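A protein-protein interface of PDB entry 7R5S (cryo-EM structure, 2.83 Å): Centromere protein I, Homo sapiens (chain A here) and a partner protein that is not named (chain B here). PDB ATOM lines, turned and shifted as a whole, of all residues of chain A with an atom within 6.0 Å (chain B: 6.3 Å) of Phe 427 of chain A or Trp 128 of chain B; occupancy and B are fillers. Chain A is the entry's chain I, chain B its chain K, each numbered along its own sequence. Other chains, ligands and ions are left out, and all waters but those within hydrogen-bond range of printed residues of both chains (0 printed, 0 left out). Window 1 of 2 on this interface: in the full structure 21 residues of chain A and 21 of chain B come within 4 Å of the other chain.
NE2 of His 374 of chain A lies close to OE1 of Glu 131 of chain B (3.5 Å). ND2 of Asn 377 of chain A lies close to NE2 of Gln 132 of chain B (3.2 Å).
O of Ser 370 of chain A is in hydrogen-bond range of ND1 of His 374 of chain A (3.2 Å). OE2 of Glu 131 of chain B lies within salt-bridge range of NH1 of Arg 127 of chain B.
CD1 of Phe 427 of chain A touches CD2 of Trp 128 of chain B (3.6 Å).
Of the printed residues of chain B, His 374 of chain A touches Glu 131. Of the printed residues of chain B, Asn 377 of chain A touches Gln 132 (3.2 Å). Phe 427 of chain A touches just one residue of chain B: Trp 128 (3.6 Å). Trp 128 of chain B touches one residue of chain A. Of the printed residues of chain A, Gln 132 of chain B touches Asn 377. The nearest residue of chain B that does not touch Phe 427 of chain A is Gln 132 of chain B (4.8 Å). The nearest residue of chain A that does not touch Trp 128 of chain B is Arg 423 of chain A (4.5 Å).
Along chain B the printed residues that touch a printed residue of chain A span positions 128 to 132. Of the 13 printed residues of chain A, 3 touch a printed residue of chain B. Among the printed residues, no Asp or Glu carboxylate lies within 4 Å of a Lys or Arg side-chain nitrogen of the other chain.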
ATOM      1  N   SER A 370      -1.054  22.397   3.601  1.00  0.00           N
ATOM      2  CA  SER A 370      -1.066  20.992   3.997  1.00  0.00           C
ATOM      3  C   SER A 370      -1.443  20.084   2.832  1.00  0.00           C
ATOM      4  O   SER A 370      -0.911  18.973   2.708  1.00  0.00           O
ATOM      5  CB  SER A 370      -2.027  20.788   5.167  1.00  0.00           C
ATOM      6  OG  SER A 370      -1.859  21.798   6.146  1.00  0.00           O
ATOM      7  N   LEU A 373       1.618  19.664   0.872  1.00  0.00           N
ATOM      8  CA  LEU A 373       2.574  18.858   1.623  1.00  0.00           C
ATOM      9  C   LEU A 373       2.235  17.377   1.519  1.00  0.00           C
ATOM     10  O   LEU A 373       3.132  16.535   1.393  1.00  0.00           O
ATOM     11  CB  LEU A 373       2.606  19.300   3.086  1.00  0.00           C
ATOM     12  CG  LEU A 373       3.398  20.566   3.416  1.00  0.00           C
ATOM     13  CD1 LEU A 373       3.234  20.933   4.881  1.00  0.00           C
ATOM     14  CD2 LEU A 373       4.866  20.385   3.075  1.00  0.00           C
ATOM     15  N   HIS A 374       0.943  17.041   1.559  1.00  0.00           N
ATOM     16  CA  HIS A 374       0.537  15.648   1.401  1.00  0.00           C
ATOM     17  C   HIS A 374       0.926  15.102   0.034  1.00  0.00           C
ATOM     18  O   HIS A 374       1.193  13.903  -0.102  1.00  0.00           O
ATOM     19  CB  HIS A 374      -0.970  15.508   1.617  1.00  0.00           C
ATOM     20  CG  HIS A 374      -1.355  15.230   3.036  1.00  0.00           C
ATOM     21  ND1 HIS A 374      -1.928  16.182   3.851  1.00  0.00           N
ATOM     22  CD2 HIS A 374      -1.246  14.108   3.786  1.00  0.00           C
ATOM     23  CE1 HIS A 374      -2.158  15.658   5.041  1.00  0.00           C
ATOM     24  NE2 HIS A 374      -1.754  14.401   5.028  1.00  0.00           N
ATOM     25  N   ASN A 377       4.871  14.777  -0.113  1.00  0.00           N
ATOM     26  CA  ASN A 377       5.375  13.755   0.798  1.00  0.00           C
ATOM     27  C   ASN A 377       5.896  12.545   0.036  1.00  0.00           C
ATOM     28  O   ASN A 377       6.917  11.959   0.412  1.00  0.00           O
ATOM     29  CB  ASN A 377       4.276  13.340   1.775  1.00  0.00           C
ATOM     30  CG  ASN A 377       4.799  12.485   2.911  1.00  0.00           C
ATOM     31  OD1 ASN A 377       6.000  12.453   3.177  1.00  0.00           O
ATOM     32  ND2 ASN A 377       3.898  11.788   3.591  1.00  0.00           N
ATOM     33  N   ILE A 422      10.677  23.855  10.750  1.00  0.00           N
ATOM     34  CA  ILE A 422      10.721  22.711  11.654  1.00  0.00           C
ATOM     35  C   ILE A 422       9.375  21.999  11.684  1.00  0.00           C
ATOM     36  O   ILE A 422       9.312  20.764  11.685  1.00  0.00           O
ATOM     37  CB  ILE A 422      11.156  23.162  13.061  1.00  0.00           C
ATOM     38  CG1 ILE A 422      12.621  23.601  13.049  1.00  0.00           C
ATOM     39  CG2 ILE A 422      10.947  22.047  14.073  1.00  0.00           C
ATOM     40  CD1 ILE A 422      13.050  24.308  14.310  1.00  0.00           C
ATOM     41  N   ARG A 423       8.279  22.761  11.705  1.00  0.00           N
ATOM     42  CA  ARG A 423       6.956  22.146  11.686  1.00  0.00           C
ATOM     43  C   ARG A 423       6.697  21.418  10.375  1.00  0.00           C
ATOM     44  O   ARG A 423       5.980  20.411  10.355  1.00  0.00           O
ATOM     45  CB  ARG A 423       5.883  23.208  11.928  1.00  0.00           C
ATOM     46  CG  ARG A 423       4.519  22.645  12.288  1.00  0.00           C
ATOM     47  CD  ARG A 423       3.450  23.727  12.301  1.00  0.00           C
ATOM     48  NE  ARG A 423       3.813  24.856  13.156  1.00  0.00           N
ATOM     49  CZ  ARG A 423       4.156  26.058  12.703  1.00  0.00           C
ATOM     50  NH1 ARG A 423       4.180  26.295  11.399  1.00  0.00           N
ATOM     51  NH2 ARG A 423       4.471  27.024  13.554  1.00  0.00           N
ATOM     52  N   ALA A 424       7.271  21.905   9.273  1.00  0.00           N
ATOM     53  CA  ALA A 424       7.097  21.231   7.991  1.00  0.00           C
ATOM     54  C   ALA A 424       7.946  19.969   7.898  1.00  0.00           C
ATOM     55  O   ALA A 424       7.506  18.966   7.326  1.00  0.00           O
ATOM     56  CB  ALA A 424       7.433  22.185   6.846  1.00  0.00           C
ATOM     57  N   GLU A 425       9.160  19.998   8.448  1.00  0.00           N
ATOM     58  CA  GLU A 425      10.050  18.847   8.382  1.00  0.00           C
ATOM     59  C   GLU A 425       9.765  17.809   9.459  1.00  0.00           C
ATOM     60  O   GLU A 425      10.272  16.686   9.361  1.00  0.00           O
ATOM     61  CB  GLU A 425      11.513  19.296   8.470  1.00  0.00           C
ATOM     62  CG  GLU A 425      11.962  19.731   9.850  1.00  0.00           C
ATOM     63  CD  GLU A 425      13.433  20.098   9.887  1.00  0.00           C
ATOM     64  OE1 GLU A 425      14.062  20.142   8.808  1.00  0.00           O
ATOM     65  OE2 GLU A 425      13.958  20.342  10.991  1.00  0.00           O
ATOM     66  N   CYS A 426       8.980  18.152  10.484  1.00  0.00           N
ATOM     67  CA  CYS A 426       8.441  17.119  11.362  1.00  0.00           C
ATOM     68  C   CYS A 426       7.496  16.209  10.591  1.00  0.00           C
ATOM     69  O   CYS A 426       7.524  14.984  10.756  1.00  0.00           O
ATOM     70  CB  CYS A 426       7.730  17.754  12.555  1.00  0.00           C
ATOM     71  SG  CYS A 426       8.817  18.156  13.943  1.00  0.00           S
ATOM     72  N   PHE A 427       6.649  16.795   9.750  1.00  0.00           N
ATOM     73  CA  PHE A 427       5.977  16.046   8.705  1.00  0.00           C
ATOM     74  C   PHE A 427       6.999  15.616   7.654  1.00  0.00           C
ATOM     75  O   PHE A 427       8.124  16.123   7.605  1.00  0.00           O
ATOM     76  CB  PHE A 427       4.872  16.893   8.072  1.00  0.00           C
ATOM     77  CG  PHE A 427       3.809  16.094   7.372  1.00  0.00           C
ATOM     78  CD1 PHE A 427       2.848  15.407   8.096  1.00  0.00           C
ATOM     79  CD2 PHE A 427       3.756  16.047   5.990  1.00  0.00           C
ATOM     80  CE1 PHE A 427       1.866  14.677   7.453  1.00  0.00           C
ATOM     81  CE2 PHE A 427       2.777  15.320   5.343  1.00  0.00           C
ATOM     82  CZ  PHE A 427       1.831  14.634   6.075  1.00  0.00           C
ATOM     83  N   LEU A 428       6.605  14.643   6.830  1.00  0.00           N
ATOM     84  CA  LEU A 428       7.441  14.049   5.784  1.00  0.00           C
ATOM     85  C   LEU A 428       8.539  13.178   6.385  1.00  0.00           C
ATOM     86  O   LEU A 428       9.224  12.451   5.658  1.00  0.00           O
ATOM     87  CB  LEU A 428       8.069  15.118   4.875  1.00  0.00           C
ATOM     88  CG  LEU A 428       7.271  16.346   4.426  1.00  0.00           C
ATOM     89  CD1 LEU A 428       8.196  17.370   3.787  1.00  0.00           C
ATOM     90  CD2 LEU A 428       6.168  15.960   3.469  1.00  0.00           C
ATOM     91  N   GLN A 429       8.691  13.230   7.711  1.00  0.00           N
ATOM     92  CA  GLN A 429       9.640  12.395   8.454  1.00  0.00           C
ATOM     93  C   GLN A 429      11.040  12.420   7.840  1.00  0.00           C
ATOM     94  O   GLN A 429      11.719  11.395   7.754  1.00  0.00           O
ATOM     95  CB  GLN A 429       9.120  10.963   8.571  1.00  0.00           C
ATOM     96  CG  GLN A 429       7.933  10.824   9.509  1.00  0.00           C
ATOM     97  CD  GLN A 429       7.291   9.457   9.440  1.00  0.00           C
ATOM     98  OE1 GLN A 429       7.289   8.708  10.416  1.00  0.00           O
ATOM     99  NE2 GLN A 429       6.734   9.125   8.282  1.00  0.00           N
ATOM    100  N   GLU A 430      11.479  13.603   7.420  1.00  0.00           N
ATOM    101  CA  GLU A 430      12.814  13.778   6.857  1.00  0.00           C
ATOM    102  C   GLU A 430      13.118  15.268   6.795  1.00  0.00           C
ATOM    103  O   GLU A 430      12.241  16.111   7.004  1.00  0.00           O
ATOM    104  CB  GLU A 430      12.935  13.139   5.470  1.00  0.00           C
ATOM    105  CG  GLU A 430      12.007  13.731   4.426  1.00  0.00           C
ATOM    106  CD  GLU A 430      12.149  13.059   3.077  1.00  0.00           C
ATOM    107  OE1 GLU A 430      13.013  12.166   2.944  1.00  0.00           O
ATOM    108  OE2 GLU A 430      11.398  13.421   2.148  1.00  0.00           O
ATOM    109  N   GLU B 123      -1.170  13.854  19.985  1.00  0.00           N
ATOM    110  CA  GLU B 123      -2.411  14.206  19.294  1.00  0.00           C
ATOM    111  C   GLU B 123      -2.152  14.530  17.823  1.00  0.00           C
ATOM    112  O   GLU B 123      -2.859  14.040  16.923  1.00  0.00           O
ATOM    113  CB  GLU B 123      -3.084  15.384  19.996  1.00  0.00           C
ATOM    114  CG  GLU B 123      -4.327  15.896  19.286  1.00  0.00           C
ATOM    115  CD  GLU B 123      -4.864  17.172  19.900  1.00  0.00           C
ATOM    116  OE1 GLU B 123      -4.217  17.706  20.827  1.00  0.00           O
ATOM    117  OE2 GLU B 123      -5.932  17.644  19.456  1.00  0.00           O
ATOM    118  N   ARG B 124      -1.136  15.359  17.561  1.00  0.00           N
ATOM    119  CA  ARG B 124      -0.852  15.748  16.179  1.00  0.00           C
ATOM    120  C   ARG B 124      -0.474  14.539  15.327  1.00  0.00           C
ATOM    121  O   ARG B 124      -0.928  14.409  14.180  1.00  0.00           O
ATOM    122  CB  ARG B 124       0.256  16.799  16.145  1.00  0.00           C
ATOM    123  CG  ARG B 124       0.262  17.639  14.879  1.00  0.00           C
ATOM    124  CD  ARG B 124       1.405  18.642  14.865  1.00  0.00           C
ATOM    125  NE  ARG B 124       1.352  19.566  15.993  1.00  0.00           N
ATOM    126  CZ  ARG B 124       2.178  19.524  17.033  1.00  0.00           C
ATOM    127  NH1 ARG B 124       3.127  18.601  17.091  1.00  0.00           N
ATOM    128  NH2 ARG B 124       2.057  20.408  18.015  1.00  0.00           N
ATOM    129  N   GLU B 125       0.353  13.643  15.872  1.00  0.00           N
ATOM    130  CA  GLU B 125       0.765  12.460  15.126  1.00  0.00           C
ATOM    131  C   GLU B 125      -0.417  11.540  14.852  1.00  0.00           C
ATOM    132  O   GLU B 125      -0.492  10.927  13.782  1.00  0.00           O
ATOM    133  CB  GLU B 125       1.860  11.712  15.888  1.00  0.00           C
ATOM    134  CG  GLU B 125       3.199  12.433  15.929  1.00  0.00           C
ATOM    135  CD  GLU B 125       3.970  12.314  14.632  1.00  0.00           C
ATOM    136  OE1 GLU B 125       3.634  11.430  13.816  1.00  0.00           O
ATOM    137  OE2 GLU B 125       4.916  13.105  14.427  1.00  0.00           O
ATOM    138  N   GLN B 126      -1.349  11.428  15.802  1.00  0.00           N
ATOM    139  CA  GLN B 126      -2.540  10.615  15.568  1.00  0.00           C
ATOM    140  C   GLN B 126      -3.355  11.163  14.401  1.00  0.00           C
ATOM    141  O   GLN B 126      -3.790  10.409  13.515  1.00  0.00           O
ATOM    142  CB  GLN B 126      -3.390  10.551  16.837  1.00  0.00           C
ATOM    143  CG  GLN B 126      -4.618   9.667  16.715  1.00  0.00           C
ATOM    144  CD  GLN B 126      -4.267   8.197  16.598  1.00  0.00           C
ATOM    145  OE1 GLN B 126      -3.497   7.667  17.397  1.00  0.00           O
ATOM    146  NE2 GLN B 126      -4.833   7.532  15.598  1.00  0.00           N
ATOM    147  N   ARG B 127      -3.576  12.482  14.386  1.00  0.00           N
ATOM    148  CA  ARG B 127      -4.327  13.075  13.278  1.00  0.00           C
ATOM    149  C   ARG B 127      -3.619  12.852  11.943  1.00  0.00           C
ATOM    150  O   ARG B 127      -4.255  12.489  10.938  1.00  0.00           O
ATOM    151  CB  ARG B 127      -4.545  14.567  13.528  1.00  0.00           C
ATOM    152  CG  ARG B 127      -5.306  15.271  12.418  1.00  0.00           C
ATOM    153  CD  ARG B 127      -5.749  16.660  12.843  1.00  0.00           C
ATOM    154  NE  ARG B 127      -4.632  17.469  13.322  1.00  0.00           N
ATOM    155  CZ  ARG B 127      -3.873  18.230  12.541  1.00  0.00           C
ATOM    156  NH1 ARG B 127      -4.108  18.287  11.238  1.00  0.00           N
ATOM    157  NH2 ARG B 127      -2.877  18.933  13.063  1.00  0.00           N
ATOM    158  N   TRP B 128      -2.299  13.065  11.914  1.00  0.00           N
ATOM    159  CA  TRP B 128      -1.543  12.858  10.682  1.00  0.00           C
ATOM    160  C   TRP B 128      -1.628  11.409  10.216  1.00  0.00           C
ATOM    161  O   TRP B 128      -1.745  11.144   9.012  1.00  0.00           O
ATOM    162  CB  TRP B 128      -0.085  13.268  10.885  1.00  0.00           C
ATOM    163  CG  TRP B 128       0.146  14.740  10.779  1.00  0.00           C
ATOM    164  CD1 TRP B 128      -0.666  15.656  10.177  1.00  0.00           C
ATOM    165  CD2 TRP B 128       1.265  15.472  11.289  1.00  0.00           C
ATOM    166  NE1 TRP B 128      -0.122  16.912  10.281  1.00  0.00           N
ATOM    167  CE2 TRP B 128       1.065  16.826  10.961  1.00  0.00           C
ATOM    168  CE3 TRP B 128       2.418  15.112  11.994  1.00  0.00           C
ATOM    169  CZ2 TRP B 128       1.974  17.822  11.311  1.00  0.00           C
ATOM    170  CZ3 TRP B 128       3.318  16.101  12.341  1.00  0.00           C
ATOM    171  CH2 TRP B 128       3.092  17.438  11.999  1.00  0.00           C
ATOM    172  N   LEU B 129      -1.564  10.459  11.152  1.00  0.00           N
ATOM    173  CA  LEU B 129      -1.660   9.049  10.791  1.00  0.00           C
ATOM    174  C   LEU B 129      -3.017   8.727  10.182  1.00  0.00           C
ATOM    175  O   LEU B 129      -3.101   7.981   9.199  1.00  0.00           O
ATOM    176  CB  LEU B 129      -1.403   8.174  12.018  1.00  0.00           C
ATOM    177  CG  LEU B 129      -1.687   6.679  11.859  1.00  0.00           C
ATOM    178  CD1 LEU B 129      -0.782   6.066  10.804  1.00  0.00           C
ATOM    179  CD2 LEU B 129      -1.531   5.958  13.188  1.00  0.00           C
ATOM    180  N   ASP B 130      -4.092   9.269  10.760  1.00  0.00           N
ATOM    181  CA  ASP B 130      -5.418   9.049  10.186  1.00  0.00           C
ATOM    182  C   ASP B 130      -5.492   9.570   8.755  1.00  0.00           C
ATOM    183  O   ASP B 130      -5.963   8.871   7.841  1.00  0.00           O
ATOM    184  CB  ASP B 130      -6.484   9.714  11.060  1.00  0.00           C
ATOM    185  CG  ASP B 130      -6.972   8.810  12.173  1.00  0.00           C
ATOM    186  OD1 ASP B 130      -7.500   9.332  13.177  1.00  0.00           O
ATOM    187  OD2 ASP B 130      -6.829   7.575  12.045  1.00  0.00           O
ATOM    188  N   GLU B 131      -5.022  10.804   8.538  1.00  0.00           N
ATOM    189  CA  GLU B 131      -5.081  11.378   7.195  1.00  0.00           C
ATOM    190  C   GLU B 131      -4.238  10.579   6.206  1.00  0.00           C
ATOM    191  O   GLU B 131      -4.644  10.368   5.054  1.00  0.00           O
ATOM    192  CB  GLU B 131      -4.636  12.839   7.230  1.00  0.00           C
ATOM    193  CG  GLU B 131      -5.582  13.748   8.000  1.00  0.00           C
ATOM    194  CD  GLU B 131      -5.162  15.202   7.956  1.00  0.00           C
ATOM    195  OE1 GLU B 131      -4.103  15.500   7.365  1.00  0.00           O
ATOM    196  OE2 GLU B 131      -5.890  16.049   8.514  1.00  0.00           O
ATOM    197  N   GLN B 132      -3.066  10.109   6.641  1.00  0.00           N
ATOM    198  CA  GLN B 132      -2.200   9.347   5.747  1.00  0.00           C
ATOM    199  C   GLN B 132      -2.805   7.988   5.417  1.00  0.00           C
ATOM    200  O   GLN B 132      -2.669   7.502   4.288  1.00  0.00           O
ATOM    201  CB  GLN B 132      -0.815   9.188   6.369  1.00  0.00           C
ATOM    202  CG  GLN B 132       0.294   8.969   5.359  1.00  0.00           C
ATOM    203  CD  GLN B 132       1.649   9.389   5.885  1.00  0.00           C
ATOM    204  OE1 GLN B 132       1.766   9.881   7.007  1.00  0.00           O
ATOM    205  NE2 GLN B 132       2.683   9.201   5.075  1.00  0.00           N
ATOM    206  N   GLN B 133      -3.473   7.357   6.388  1.00  0.00           N
ATOM    207  CA  GLN B 133      -4.188   6.117   6.105  1.00  0.00           C
ATOM    208  C   GLN B 133      -5.268   6.336   5.056  1.00  0.00           C
ATOM    209  O   GLN B 133      -5.415   5.533   4.123  1.00  0.00           O
ATOM    210  CB  GLN B 133      -4.801   5.556   7.388  1.00  0.00           C
ATOM    211  CG  GLN B 133      -3.986   4.460   8.049  1.00  0.00           C
ATOM    212  CD  GLN B 133      -4.631   3.941   9.318  1.00  0.00           C
ATOM    213  OE1 GLN B 133      -5.590   4.524   9.823  1.00  0.00           O
ATOM    214  NE2 GLN B 133      -4.104   2.841   9.841  1.00  0.00           N
